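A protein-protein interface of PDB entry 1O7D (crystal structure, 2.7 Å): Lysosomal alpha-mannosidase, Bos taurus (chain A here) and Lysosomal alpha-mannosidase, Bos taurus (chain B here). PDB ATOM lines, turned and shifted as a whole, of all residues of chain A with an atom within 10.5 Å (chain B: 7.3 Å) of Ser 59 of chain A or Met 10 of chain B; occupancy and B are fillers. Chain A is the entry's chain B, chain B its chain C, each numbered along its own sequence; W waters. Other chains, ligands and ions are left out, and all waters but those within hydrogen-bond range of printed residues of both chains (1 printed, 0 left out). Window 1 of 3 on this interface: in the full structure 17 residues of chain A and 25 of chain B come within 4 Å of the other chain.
OH of Tyr 55 of chain A lies close to N of Ser 36 of chain B, at 3.4 Å. The side-chain sulfur (SD) of Met 10 of chain B lies close to the backbone carbonyl oxygen (O) of Glu 56 of chain A (3.7 Å). NE1 of Trp 39 of chain B lies within hydrogen-bond range of OG of Ser 59 of chain A, at 2.9 Å.
The side-chain amide nitrogen (NE2) of Gln 64 of chain A lies within hydrogen-bond range of the side-chain hydroxyl (OH) of Tyr 60 of chain A (2.5 Å). The side-chain hydroxyl (OG) of Ser 59 of chain A lies within hydrogen-bond range of the backbone carbonyl oxygen (O) of Tyr 55 of chain A, at 2.9 Å. O of Leu 63 of chain A sits close to ND2 of Asn 67 of chain A (3.3 Å).
Leu 35 of chain B touches Tyr 55 of chain A. Tyr 55 of chain A touches Trp 39 of chain B (CE2 to NE1, 3.9 Å). Glu 56 of chain A touches Gln 14 of chain B (OE2 to NE2, 3.5 Å). CB of Ser 59 of chain A touches SD of Met 10 of chain B, 3.7 Å away. Ser 59 of chain A touches Leu 35 of chain B. Met 10 of chain B touches Tyr 60 of chain A (SD to N, 3.9 Å). Leu 6 of chain B touches Phe 62 of chain A. Trp 39 of chain B touches Phe 62 of chain A (CE3 to CE2, 3.6 Å). CD2 of Leu 6 of chain B touches CA of Leu 63 of chain A, at 3.6 Å. Leu 63 of chain A touches Asn 7 of chain B.
Of chain B, only Met 10, Leu 35 and Trp 39 come within 4 Å of Ser 59 of chain A. Of chain A, only Phe 62 and Leu 63 come within 4 Å of Leu 6 of chain B. No residue of chain A comes within 4 Å of Ala 9 of chain B. No residue of chain A comes within 4 Å of Ala 11 of chain B. Leu 13 of chain B touches none of the printed residues of chain A. Printed residues of chain A within 4 Å of Leu 35 of chain B: Tyr 55 (3.8 Å) and Ser 59 (3.4 Å). Printed residues of chain B within 4 Å of Glu 56 of chain A: Met 10 (3.7 Å) and Gln 14 (3.5 Å). Of the printed residues of chain B, Leu 63 of chain A touches Leu 6 (3.6 Å) and Asn 7 (3.6 Å). Printed residues of chain B within 4 Å of Tyr 55 of chain A: Leu 35 (3.8 Å), Ser 36 (3.3 Å) and Trp 39 (3.9 Å). Asn 67 of chain A touches none of the printed residues of chain B. The nearest residue of chain A that does not touch Met 10 of chain B is Leu 63 of chain A (4.3 Å). The nearest printed residue of chain A that does not touch Leu 35 of chain B is Glu 56 of chain A (4.2 Å).
Of the 16 printed residues of chain B, 7 touch a printed residue of chain A. Along chain A the printed residues that touch a printed residue of chain B span positions 55 to 63. Among the printed residues, no Asp or Glu carboxylate lies within 4 Å of a Lys or Arg side-chain nitrogen of the other chain.
Water W1 lies within hydrogen-bond range of the side-chain carboxylate of Glu 56 of chain A and the side-chain amide nitrogen of Gln 14 of chain B.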
ATOM      1  N   ALA A  51     -15.030   8.914   6.946  1.00  0.00           N
ATOM      2  CA  ALA A  51     -15.085   8.794   8.393  1.00  0.00           C
ATOM      3  C   ALA A  51     -14.137   7.734   8.912  1.00  0.00           C
ATOM      4  O   ALA A  51     -13.234   8.033   9.687  1.00  0.00           O
ATOM      5  CB  ALA A  51     -16.485   8.473   8.826  1.00  0.00           C
ATOM      6  N   LEU A  52     -14.339   6.493   8.491  1.00  0.00           N
ATOM      7  CA  LEU A  52     -13.469   5.427   8.950  1.00  0.00           C
ATOM      8  C   LEU A  52     -12.014   5.725   8.625  1.00  0.00           C
ATOM      9  O   LEU A  52     -11.139   5.592   9.481  1.00  0.00           O
ATOM     10  CB  LEU A  52     -13.859   4.093   8.319  1.00  0.00           C
ATOM     11  CG  LEU A  52     -13.072   2.896   8.858  1.00  0.00           C
ATOM     12  CD1 LEU A  52     -13.146   2.849  10.377  1.00  0.00           C
ATOM     13  CD2 LEU A  52     -13.640   1.639   8.267  1.00  0.00           C
ATOM     14  N   LYS A  53     -11.760   6.130   7.385  1.00  0.00           N
ATOM     15  CA  LYS A  53     -10.400   6.428   6.977  1.00  0.00           C
ATOM     16  C   LYS A  53      -9.725   7.365   7.976  1.00  0.00           C
ATOM     17  O   LYS A  53      -8.580   7.146   8.352  1.00  0.00           O
ATOM     18  CB  LYS A  53     -10.385   7.017   5.562  1.00  0.00           C
ATOM     19  CG  LYS A  53     -10.265   5.964   4.458  1.00  0.00           C
ATOM     20  CD  LYS A  53     -10.480   6.556   3.056  1.00  0.00           C
ATOM     21  CE  LYS A  53     -10.069   5.590   1.931  1.00  0.00           C
ATOM     22  NZ  LYS A  53     -10.953   4.410   1.771  1.00  0.00           N
ATOM     23  N   ARG A  54     -10.447   8.385   8.426  1.00  0.00           N
ATOM     24  CA  ARG A  54      -9.921   9.344   9.393  1.00  0.00           C
ATOM     25  C   ARG A  54      -9.797   8.750  10.798  1.00  0.00           C
ATOM     26  O   ARG A  54      -8.856   9.059  11.527  1.00  0.00           O
ATOM     27  CB  ARG A  54     -10.826  10.582   9.434  1.00  0.00           C
ATOM     28  CG  ARG A  54     -10.486  11.586  10.525  1.00  0.00           C
ATOM     29  CD  ARG A  54      -9.071  12.132  10.384  1.00  0.00           C
ATOM     30  NE  ARG A  54      -8.606  12.763  11.619  1.00  0.00           N
ATOM     31  CZ  ARG A  54      -7.394  13.286  11.784  1.00  0.00           C
ATOM     32  NH1 ARG A  54      -6.518  13.260  10.787  1.00  0.00           N
ATOM     33  NH2 ARG A  54      -7.057  13.823  12.950  1.00  0.00           N
ATOM     34  N   TYR A  55     -10.752   7.904  11.170  1.00  0.00           N
ATOM     35  CA  TYR A  55     -10.757   7.274  12.485  1.00  0.00           C
ATOM     36  C   TYR A  55      -9.499   6.450  12.675  1.00  0.00           C
ATOM     37  O   TYR A  55      -8.940   6.398  13.766  1.00  0.00           O
ATOM     38  CB  TYR A  55     -11.974   6.360  12.635  1.00  0.00           C
ATOM     39  CG  TYR A  55     -12.178   5.823  14.034  1.00  0.00           C
ATOM     40  CD1 TYR A  55     -13.048   4.768  14.275  1.00  0.00           C
ATOM     41  CD2 TYR A  55     -11.527   6.392  15.123  1.00  0.00           C
ATOM     42  CE1 TYR A  55     -13.264   4.298  15.556  1.00  0.00           C
ATOM     43  CE2 TYR A  55     -11.737   5.927  16.407  1.00  0.00           C
ATOM     44  CZ  TYR A  55     -12.606   4.883  16.614  1.00  0.00           C
ATOM     45  OH  TYR A  55     -12.823   4.425  17.888  1.00  0.00           O
ATOM     46  N   GLU A  56      -9.057   5.804  11.604  1.00  0.00           N
ATOM     47  CA  GLU A  56      -7.869   4.977  11.664  1.00  0.00           C
ATOM     48  C   GLU A  56      -6.603   5.807  11.697  1.00  0.00           C
ATOM     49  O   GLU A  56      -5.785   5.627  12.597  1.00  0.00           O
ATOM     50  CB  GLU A  56      -7.842   3.993  10.487  1.00  0.00           C
ATOM     51  CG  GLU A  56      -6.536   3.237  10.288  1.00  0.00           C
ATOM     52  CD  GLU A  56      -5.556   4.006   9.406  1.00  0.00           C
ATOM     53  OE1 GLU A  56      -5.969   5.050   8.851  1.00  0.00           O
ATOM     54  OE2 GLU A  56      -4.388   3.583   9.253  1.00  0.00           O
ATOM     55  N   ARG A  57      -6.432   6.731  10.754  1.00  0.00           N
ATOM     56  CA  ARG A  57      -5.201   7.515  10.760  1.00  0.00           C
ATOM     57  C   ARG A  57      -5.044   8.291  12.057  1.00  0.00           C
ATOM     58  O   ARG A  57      -3.963   8.781  12.367  1.00  0.00           O
ATOM     59  CB  ARG A  57      -5.103   8.490   9.577  1.00  0.00           C
ATOM     60  CG  ARG A  57      -3.659   8.950   9.412  1.00  0.00           C
ATOM     61  CD  ARG A  57      -3.429  10.239   8.651  1.00  0.00           C
ATOM     62  NE  ARG A  57      -3.413  10.125   7.186  1.00  0.00           N
ATOM     63  CZ  ARG A  57      -3.211   9.012   6.482  1.00  0.00           C
ATOM     64  NH1 ARG A  57      -3.001   7.836   7.076  1.00  0.00           N
ATOM     65  NH2 ARG A  57      -3.206   9.084   5.158  1.00  0.00           N
ATOM     66  N   LEU A  58      -6.132   8.395  12.807  1.00  0.00           N
ATOM     67  CA  LEU A  58      -6.131   9.100  14.078  1.00  0.00           C
ATOM     68  C   LEU A  58      -5.731   8.128  15.168  1.00  0.00           C
ATOM     69  O   LEU A  58      -4.981   8.479  16.079  1.00  0.00           O
ATOM     70  CB  LEU A  58      -7.517   9.658  14.368  1.00  0.00           C
ATOM     71  CG  LEU A  58      -7.759  10.307  15.731  1.00  0.00           C
ATOM     72  CD1 LEU A  58      -6.865  11.522  15.899  1.00  0.00           C
ATOM     73  CD2 LEU A  58      -9.239  10.683  15.838  1.00  0.00           C
ATOM     74  N   SER A  59      -6.236   6.902  15.077  1.00  0.00           N
ATOM     75  CA  SER A  59      -5.897   5.891  16.067  1.00  0.00           C
ATOM     76  C   SER A  59      -4.379   5.641  16.016  1.00  0.00           C
ATOM     77  O   SER A  59      -3.751   5.253  17.024  1.00  0.00           O
ATOM     78  CB  SER A  59      -6.670   4.597  15.798  1.00  0.00           C
ATOM     79  OG  SER A  59      -8.058   4.777  15.987  1.00  0.00           O
ATOM     80  N   TYR A  60      -3.791   5.871  14.843  1.00  0.00           N
ATOM     81  CA  TYR A  60      -2.355   5.703  14.683  1.00  0.00           C
ATOM     82  C   TYR A  60      -1.627   6.712  15.589  1.00  0.00           C
ATOM     83  O   TYR A  60      -0.800   6.340  16.427  1.00  0.00           O
ATOM     84  CB  TYR A  60      -1.936   5.933  13.227  1.00  0.00           C
ATOM     85  CG  TYR A  60      -0.427   5.876  13.031  1.00  0.00           C
ATOM     86  CD1 TYR A  60       0.246   4.651  12.939  1.00  0.00           C
ATOM     87  CD2 TYR A  60       0.329   7.051  12.973  1.00  0.00           C
ATOM     88  CE1 TYR A  60       1.628   4.605  12.795  1.00  0.00           C
ATOM     89  CE2 TYR A  60       1.709   7.012  12.831  1.00  0.00           C
ATOM     90  CZ  TYR A  60       2.355   5.790  12.742  1.00  0.00           C
ATOM     91  OH  TYR A  60       3.723   5.764  12.587  1.00  0.00           O
ATOM     92  N   ASN A  61      -1.949   7.990  15.404  1.00  0.00           N
ATOM     93  CA  ASN A  61      -1.355   9.070  16.174  1.00  0.00           C
ATOM     94  C   ASN A  61      -1.489   8.734  17.638  1.00  0.00           C
ATOM     95  O   ASN A  61      -0.583   8.978  18.428  1.00  0.00           O
ATOM     96  CB  ASN A  61      -2.094  10.378  15.893  1.00  0.00           C
ATOM     97  CG  ASN A  61      -1.346  11.593  16.395  1.00  0.00           C
ATOM     98  OD1 ASN A  61      -1.771  12.731  16.192  1.00  0.00           O
ATOM     99  ND2 ASN A  61      -0.222  11.359  17.043  1.00  0.00           N
ATOM    100  N   PHE A  62      -2.637   8.157  17.975  1.00  0.00           N
ATOM    101  CA  PHE A  62      -2.967   7.798  19.343  1.00  0.00           C
ATOM    102  C   PHE A  62      -2.165   6.620  19.887  1.00  0.00           C
ATOM    103  O   PHE A  62      -1.606   6.705  20.981  1.00  0.00           O
ATOM    104  CB  PHE A  62      -4.473   7.512  19.454  1.00  0.00           C
ATOM    105  CG  PHE A  62      -4.965   7.379  20.871  1.00  0.00           C
ATOM    106  CD1 PHE A  62      -4.961   8.473  21.723  1.00  0.00           C
ATOM    107  CD2 PHE A  62      -5.390   6.150  21.364  1.00  0.00           C
ATOM    108  CE1 PHE A  62      -5.370   8.344  23.051  1.00  0.00           C
ATOM    109  CE2 PHE A  62      -5.805   6.005  22.695  1.00  0.00           C
ATOM    110  CZ  PHE A  62      -5.792   7.100  23.539  1.00  0.00           C
ATOM    111  N   LEU A  63      -2.119   5.525  19.137  1.00  0.00           N
ATOM    112  CA  LEU A  63      -1.371   4.349  19.568  1.00  0.00           C
ATOM    113  C   LEU A  63       0.091   4.749  19.821  1.00  0.00           C
ATOM    114  O   LEU A  63       0.727   4.292  20.773  1.00  0.00           O
ATOM    115  CB  LEU A  63      -1.424   3.278  18.477  1.00  0.00           C
ATOM    116  CG  LEU A  63      -1.244   1.786  18.793  1.00  0.00           C
ATOM    117  CD1 LEU A  63      -0.651   1.135  17.560  1.00  0.00           C
ATOM    118  CD2 LEU A  63      -0.345   1.558  19.978  1.00  0.00           C
ATOM    119  N   GLN A  64       0.613   5.602  18.949  1.00  0.00           N
ATOM    120  CA  GLN A  64       1.980   6.086  19.050  1.00  0.00           C
ATOM    121  C   GLN A  64       2.210   6.733  20.405  1.00  0.00           C
ATOM    122  O   GLN A  64       3.109   6.347  21.146  1.00  0.00           O
ATOM    123  CB  GLN A  64       2.246   7.116  17.966  1.00  0.00           C
ATOM    124  CG  GLN A  64       3.537   6.877  17.263  1.00  0.00           C
ATOM    125  CD  GLN A  64       3.439   5.736  16.286  1.00  0.00           C
ATOM    126  OE1 GLN A  64       2.878   4.671  16.589  1.00  0.00           O
ATOM    127  NE2 GLN A  64       3.996   5.943  15.097  1.00  0.00           N
ATOM    128  N   VAL A  65       1.401   7.742  20.700  1.00  0.00           N
ATOM    129  CA  VAL A  65       1.476   8.444  21.961  1.00  0.00           C
ATOM    130  C   VAL A  65       1.380   7.417  23.067  1.00  0.00           C
ATOM    131  O   VAL A  65       2.108   7.480  24.038  1.00  0.00           O
ATOM    132  CB  VAL A  65       0.318   9.445  22.079  1.00  0.00           C
ATOM    133  CG1 VAL A  65       0.295  10.063  23.448  1.00  0.00           C
ATOM    134  CG2 VAL A  65       0.464  10.526  21.006  1.00  0.00           C
ATOM    135  N   CYS A  66       0.479   6.457  22.908  1.00  0.00           N
ATOM    136  CA  CYS A  66       0.303   5.394  23.897  1.00  0.00           C
ATOM    137  C   CYS A  66       1.629   4.640  24.047  1.00  0.00           C
ATOM    138  O   CYS A  66       2.102   4.432  25.163  1.00  0.00           O
ATOM    139  CB  CYS A  66      -0.822   4.434  23.451  1.00  0.00           C
ATOM    140  SG  CYS A  66      -1.352   3.094  24.607  1.00  0.00           S
ATOM    141  N   ASN A  67       2.230   4.247  22.924  1.00  0.00           N
ATOM    142  CA  ASN A  67       3.501   3.533  22.947  1.00  0.00           C
ATOM    143  C   ASN A  67       4.594   4.324  23.639  1.00  0.00           C
ATOM    144  O   ASN A  67       5.242   3.820  24.558  1.00  0.00           O
ATOM    145  CB  ASN A  67       3.970   3.205  21.531  1.00  0.00           C
ATOM    146  CG  ASN A  67       3.293   1.986  20.969  1.00  0.00           C
ATOM    147  OD1 ASN A  67       3.128   0.985  21.672  1.00  0.00           O
ATOM    148  ND2 ASN A  67       2.904   2.050  19.702  1.00  0.00           N
ATOM    149  N   ALA B   4      -1.750  -3.329  23.823  1.00  0.00           N
ATOM    150  CA  ALA B   4      -1.871  -4.464  22.891  1.00  0.00           C
ATOM    151  C   ALA B   4      -3.153  -4.447  22.061  1.00  0.00           C
ATOM    152  O   ALA B   4      -3.117  -4.610  20.837  1.00  0.00           O
ATOM    153  CB  ALA B   4      -1.765  -5.791  23.651  1.00  0.00           C
ATOM    154  N   PRO B   5      -4.307  -4.260  22.722  1.00  0.00           N
ATOM    155  CA  PRO B   5      -5.582  -4.227  22.005  1.00  0.00           C
ATOM    156  C   PRO B   5      -5.666  -3.193  20.878  1.00  0.00           C
ATOM    157  O   PRO B   5      -6.202  -3.474  19.813  1.00  0.00           O
ATOM    158  CB  PRO B   5      -6.596  -3.991  23.120  1.00  0.00           C
ATOM    159  CG  PRO B   5      -5.760  -3.353  24.223  1.00  0.00           C
ATOM    160  CD  PRO B   5      -4.519  -4.140  24.175  1.00  0.00           C
ATOM    161  N   LEU B   6      -5.127  -2.007  21.091  1.00  0.00           N
ATOM    162  CA  LEU B   6      -5.195  -1.017  20.046  1.00  0.00           C
ATOM    163  C   LEU B   6      -4.220  -1.310  18.904  1.00  0.00           C
ATOM    164  O   LEU B   6      -4.537  -1.046  17.742  1.00  0.00           O
ATOM    165  CB  LEU B   6      -4.927   0.365  20.623  1.00  0.00           C
ATOM    166  CG  LEU B   6      -5.010   1.509  19.622  1.00  0.00           C
ATOM    167  CD1 LEU B   6      -6.437   1.646  19.128  1.00  0.00           C
ATOM    168  CD2 LEU B   6      -4.546   2.793  20.275  1.00  0.00           C
ATOM    169  N   ASN B   7      -3.042  -1.853  19.223  1.00  0.00           N
ATOM    170  CA  ASN B   7      -2.024  -2.178  18.204  1.00  0.00           C
ATOM    171  C   ASN B   7      -2.549  -3.238  17.253  1.00  0.00           C
ATOM    172  O   ASN B   7      -2.238  -3.254  16.063  1.00  0.00           O
ATOM    173  CB  ASN B   7      -0.750  -2.721  18.853  1.00  0.00           C
ATOM    174  CG  ASN B   7       0.358  -2.992  17.838  1.00  0.00           C
ATOM    175  OD1 ASN B   7       1.026  -2.071  17.348  1.00  0.00           O
ATOM    176  ND2 ASN B   7       0.552  -4.259  17.517  1.00  0.00           N
ATOM    177  N   GLU B   8      -3.346  -4.132  17.817  1.00  0.00           N
ATOM    178  CA  GLU B   8      -3.970  -5.226  17.095  1.00  0.00           C
ATOM    179  C   GLU B   8      -5.088  -4.739  16.161  1.00  0.00           C
ATOM    180  O   GLU B   8      -5.167  -5.165  15.017  1.00  0.00           O
ATOM    181  CB  GLU B   8      -4.540  -6.203  18.107  1.00  0.00           C
ATOM    182  CG  GLU B   8      -4.796  -7.559  17.548  1.00  0.00           C
ATOM    183  CD  GLU B   8      -5.296  -8.513  18.600  1.00  0.00           C
ATOM    184  OE1 GLU B   8      -4.600  -8.648  19.633  1.00  0.00           O
ATOM    185  OE2 GLU B   8      -6.373  -9.128  18.391  1.00  0.00           O
ATOM    186  N   ALA B   9      -5.955  -3.854  16.662  1.00  0.00           N
ATOM    187  CA  ALA B   9      -7.060  -3.310  15.882  1.00  0.00           C
ATOM    188  C   ALA B   9      -6.539  -2.448  14.722  1.00  0.00           C
ATOM    189  O   ALA B   9      -7.113  -2.433  13.627  1.00  0.00           O
ATOM    190  CB  ALA B   9      -7.995  -2.501  16.786  1.00  0.00           C
ATOM    191  N   MET B  10      -5.451  -1.724  14.964  1.00  0.00           N
ATOM    192  CA  MET B  10      -4.839  -0.912  13.920  1.00  0.00           C
ATOM    193  C   MET B  10      -4.288  -1.836  12.829  1.00  0.00           C
ATOM    194  O   MET B  10      -4.209  -1.474  11.662  1.00  0.00           O
ATOM    195  CB  MET B  10      -3.705  -0.080  14.501  1.00  0.00           C
ATOM    196  CG  MET B  10      -4.136   1.236  15.052  1.00  0.00           C
ATOM    197  SD  MET B  10      -4.706   2.235  13.725  1.00  0.00           S
ATOM    198  CE  MET B  10      -3.208   2.256  12.631  1.00  0.00           C
ATOM    199  N   ALA B  11      -3.888  -3.038  13.219  1.00  0.00           N
ATOM    200  CA  ALA B  11      -3.379  -3.993  12.253  1.00  0.00           C
ATOM    201  C   ALA B  11      -4.552  -4.479  11.398  1.00  0.00           C
ATOM    202  O   ALA B  11      -4.481  -4.485  10.170  1.00  0.00           O
ATOM    203  CB  ALA B  11      -2.720  -5.173  12.979  1.00  0.00           C
ATOM    204  N   VAL B  12      -5.636  -4.875  12.060  1.00  0.00           N
ATOM    205  CA  VAL B  12      -6.820  -5.361  11.377  1.00  0.00           C
ATOM    206  C   VAL B  12      -7.283  -4.348  10.346  1.00  0.00           C
ATOM    207  O   VAL B  12      -7.500  -4.681   9.179  1.00  0.00           O
ATOM    208  CB  VAL B  12      -7.982  -5.609  12.364  1.00  0.00           C
ATOM    209  CG1 VAL B  12      -9.220  -6.063  11.610  1.00  0.00           C
ATOM    210  CG2 VAL B  12      -7.588  -6.659  13.381  1.00  0.00           C
ATOM    211  N   LEU B  13      -7.428  -3.102  10.770  1.00  0.00           N
ATOM    212  CA  LEU B  13      -7.893  -2.089   9.850  1.00  0.00           C
ATOM    213  C   LEU B  13      -6.959  -1.901   8.662  1.00  0.00           C
ATOM    214  O   LEU B  13      -7.302  -1.240   7.680  1.00  0.00           O
ATOM    215  CB  LEU B  13      -8.091  -0.771  10.586  1.00  0.00           C
ATOM    216  CG  LEU B  13      -9.167  -0.768  11.675  1.00  0.00           C
ATOM    217  CD1 LEU B  13      -9.192   0.606  12.189  1.00  0.00           C
ATOM    218  CD2 LEU B  13     -10.547  -1.111  11.179  1.00  0.00           C
ATOM    219  N   GLN B  14      -5.780  -2.491   8.728  1.00  0.00           N
ATOM    220  CA  GLN B  14      -4.851  -2.340   7.635  1.00  0.00           C
ATOM    221  C   GLN B  14      -5.177  -3.298   6.524  1.00  0.00           C
ATOM    222  O   GLN B  14      -4.583  -3.242   5.454  1.00  0.00           O
ATOM    223  CB  GLN B  14      -3.432  -2.554   8.134  1.00  0.00           C
ATOM    224  CG  GLN B  14      -3.032  -1.500   9.129  1.00  0.00           C
ATOM    225  CD  GLN B  14      -3.121  -0.120   8.537  1.00  0.00           C
ATOM    226  OE1 GLN B  14      -3.947   0.145   7.673  1.00  0.00           O
ATOM    227  NE2 GLN B  14      -2.277   0.768   9.000  1.00  0.00           N
ATOM    228  N   HIS B  15      -6.128  -4.189   6.767  1.00  0.00           N
ATOM    229  CA  HIS B  15      -6.549  -5.155   5.750  1.00  0.00           C
ATOM    230  C   HIS B  15      -6.852  -4.412   4.437  1.00  0.00           C
ATOM    231  O   HIS B  15      -6.903  -3.178   4.422  1.00  0.00           O
ATOM    232  CB  HIS B  15      -7.806  -5.869   6.236  1.00  0.00           C
ATOM    233  CG  HIS B  15      -8.318  -6.903   5.264  1.00  0.00           C
ATOM    234  ND1 HIS B  15      -7.613  -8.043   4.957  1.00  0.00           N
ATOM    235  CD2 HIS B  15      -9.448  -6.931   4.530  1.00  0.00           C
ATOM    236  CE1 HIS B  15      -8.301  -8.742   4.059  1.00  0.00           C
ATOM    237  NE2 HIS B  15      -9.408  -8.095   3.785  1.00  0.00           N
ATOM    238  N   GLN B  34     -13.839  -2.550  16.976  1.00  0.00           N
ATOM    239  CA  GLN B  34     -12.561  -3.083  17.475  1.00  0.00           C
ATOM    240  C   GLN B  34     -11.623  -1.946  17.866  1.00  0.00           C
ATOM    241  O   GLN B  34     -10.847  -2.079  18.811  1.00  0.00           O
ATOM    242  CB  GLN B  34     -11.852  -3.963  16.426  1.00  0.00           C
ATOM    243  CG  GLN B  34     -12.410  -5.373  16.261  1.00  0.00           C
ATOM    244  CD  GLN B  34     -11.695  -6.168  15.156  1.00  0.00           C
ATOM    245  OE1 GLN B  34     -10.511  -6.526  15.287  1.00  0.00           O
ATOM    246  NE2 GLN B  34     -12.412  -6.440  14.058  1.00  0.00           N
ATOM    247  N   LEU B  35     -11.685  -0.842  17.123  1.00  0.00           N
ATOM    248  CA  LEU B  35     -10.857   0.325  17.405  1.00  0.00           C
ATOM    249  C   LEU B  35     -11.292   1.054  18.661  1.00  0.00           C
ATOM    250  O   LEU B  35     -10.467   1.510  19.436  1.00  0.00           O
ATOM    251  CB  LEU B  35     -10.932   1.321  16.266  1.00  0.00           C
ATOM    252  CG  LEU B  35     -10.020   1.133  15.076  1.00  0.00           C
ATOM    253  CD1 LEU B  35      -9.962   2.467  14.354  1.00  0.00           C
ATOM    254  CD2 LEU B  35      -8.633   0.703  15.520  1.00  0.00           C
ATOM    255  N   SER B  36     -12.597   1.202  18.833  1.00  0.00           N
ATOM    256  CA  SER B  36     -13.116   1.887  19.998  1.00  0.00           C
ATOM    257  C   SER B  36     -12.657   1.148  21.253  1.00  0.00           C
ATOM    258  O   SER B  36     -12.174   1.749  22.214  1.00  0.00           O
ATOM    259  CB  SER B  36     -14.648   1.936  19.937  1.00  0.00           C
ATOM    260  OG  SER B  36     -15.190   2.727  20.979  1.00  0.00           O
ATOM    261  N   TRP B  39      -9.034   1.749  22.411  1.00  0.00           N
ATOM    262  CA  TRP B  39      -8.740   3.067  22.962  1.00  0.00           C
ATOM    263  C   TRP B  39      -8.856   3.138  24.482  1.00  0.00           C
ATOM    264  O   TRP B  39      -8.221   3.972  25.113  1.00  0.00           O
ATOM    265  CB  TRP B  39      -9.675   4.117  22.350  1.00  0.00           C
ATOM    266  CG  TRP B  39      -9.267   4.685  20.998  1.00  0.00           C
ATOM    267  CD1 TRP B  39      -9.156   4.013  19.810  1.00  0.00           C
ATOM    268  CD2 TRP B  39      -9.004   6.064  20.700  1.00  0.00           C
ATOM    269  NE1 TRP B  39      -8.846   4.887  18.794  1.00  0.00           N
ATOM    270  CE2 TRP B  39      -8.746   6.150  19.310  1.00  0.00           C
ATOM    271  CE3 TRP B  39      -8.957   7.231  21.472  1.00  0.00           C
ATOM    272  CZ2 TRP B  39      -8.452   7.359  18.678  1.00  0.00           C
ATOM    273  CZ3 TRP B  39      -8.664   8.427  20.847  1.00  0.00           C
ATOM    274  CH2 TRP B  39      -8.413   8.483  19.459  1.00  0.00           C
HETATM  275  O   HOH W   1      -2.879   3.229   7.257  1.00  0.00           O
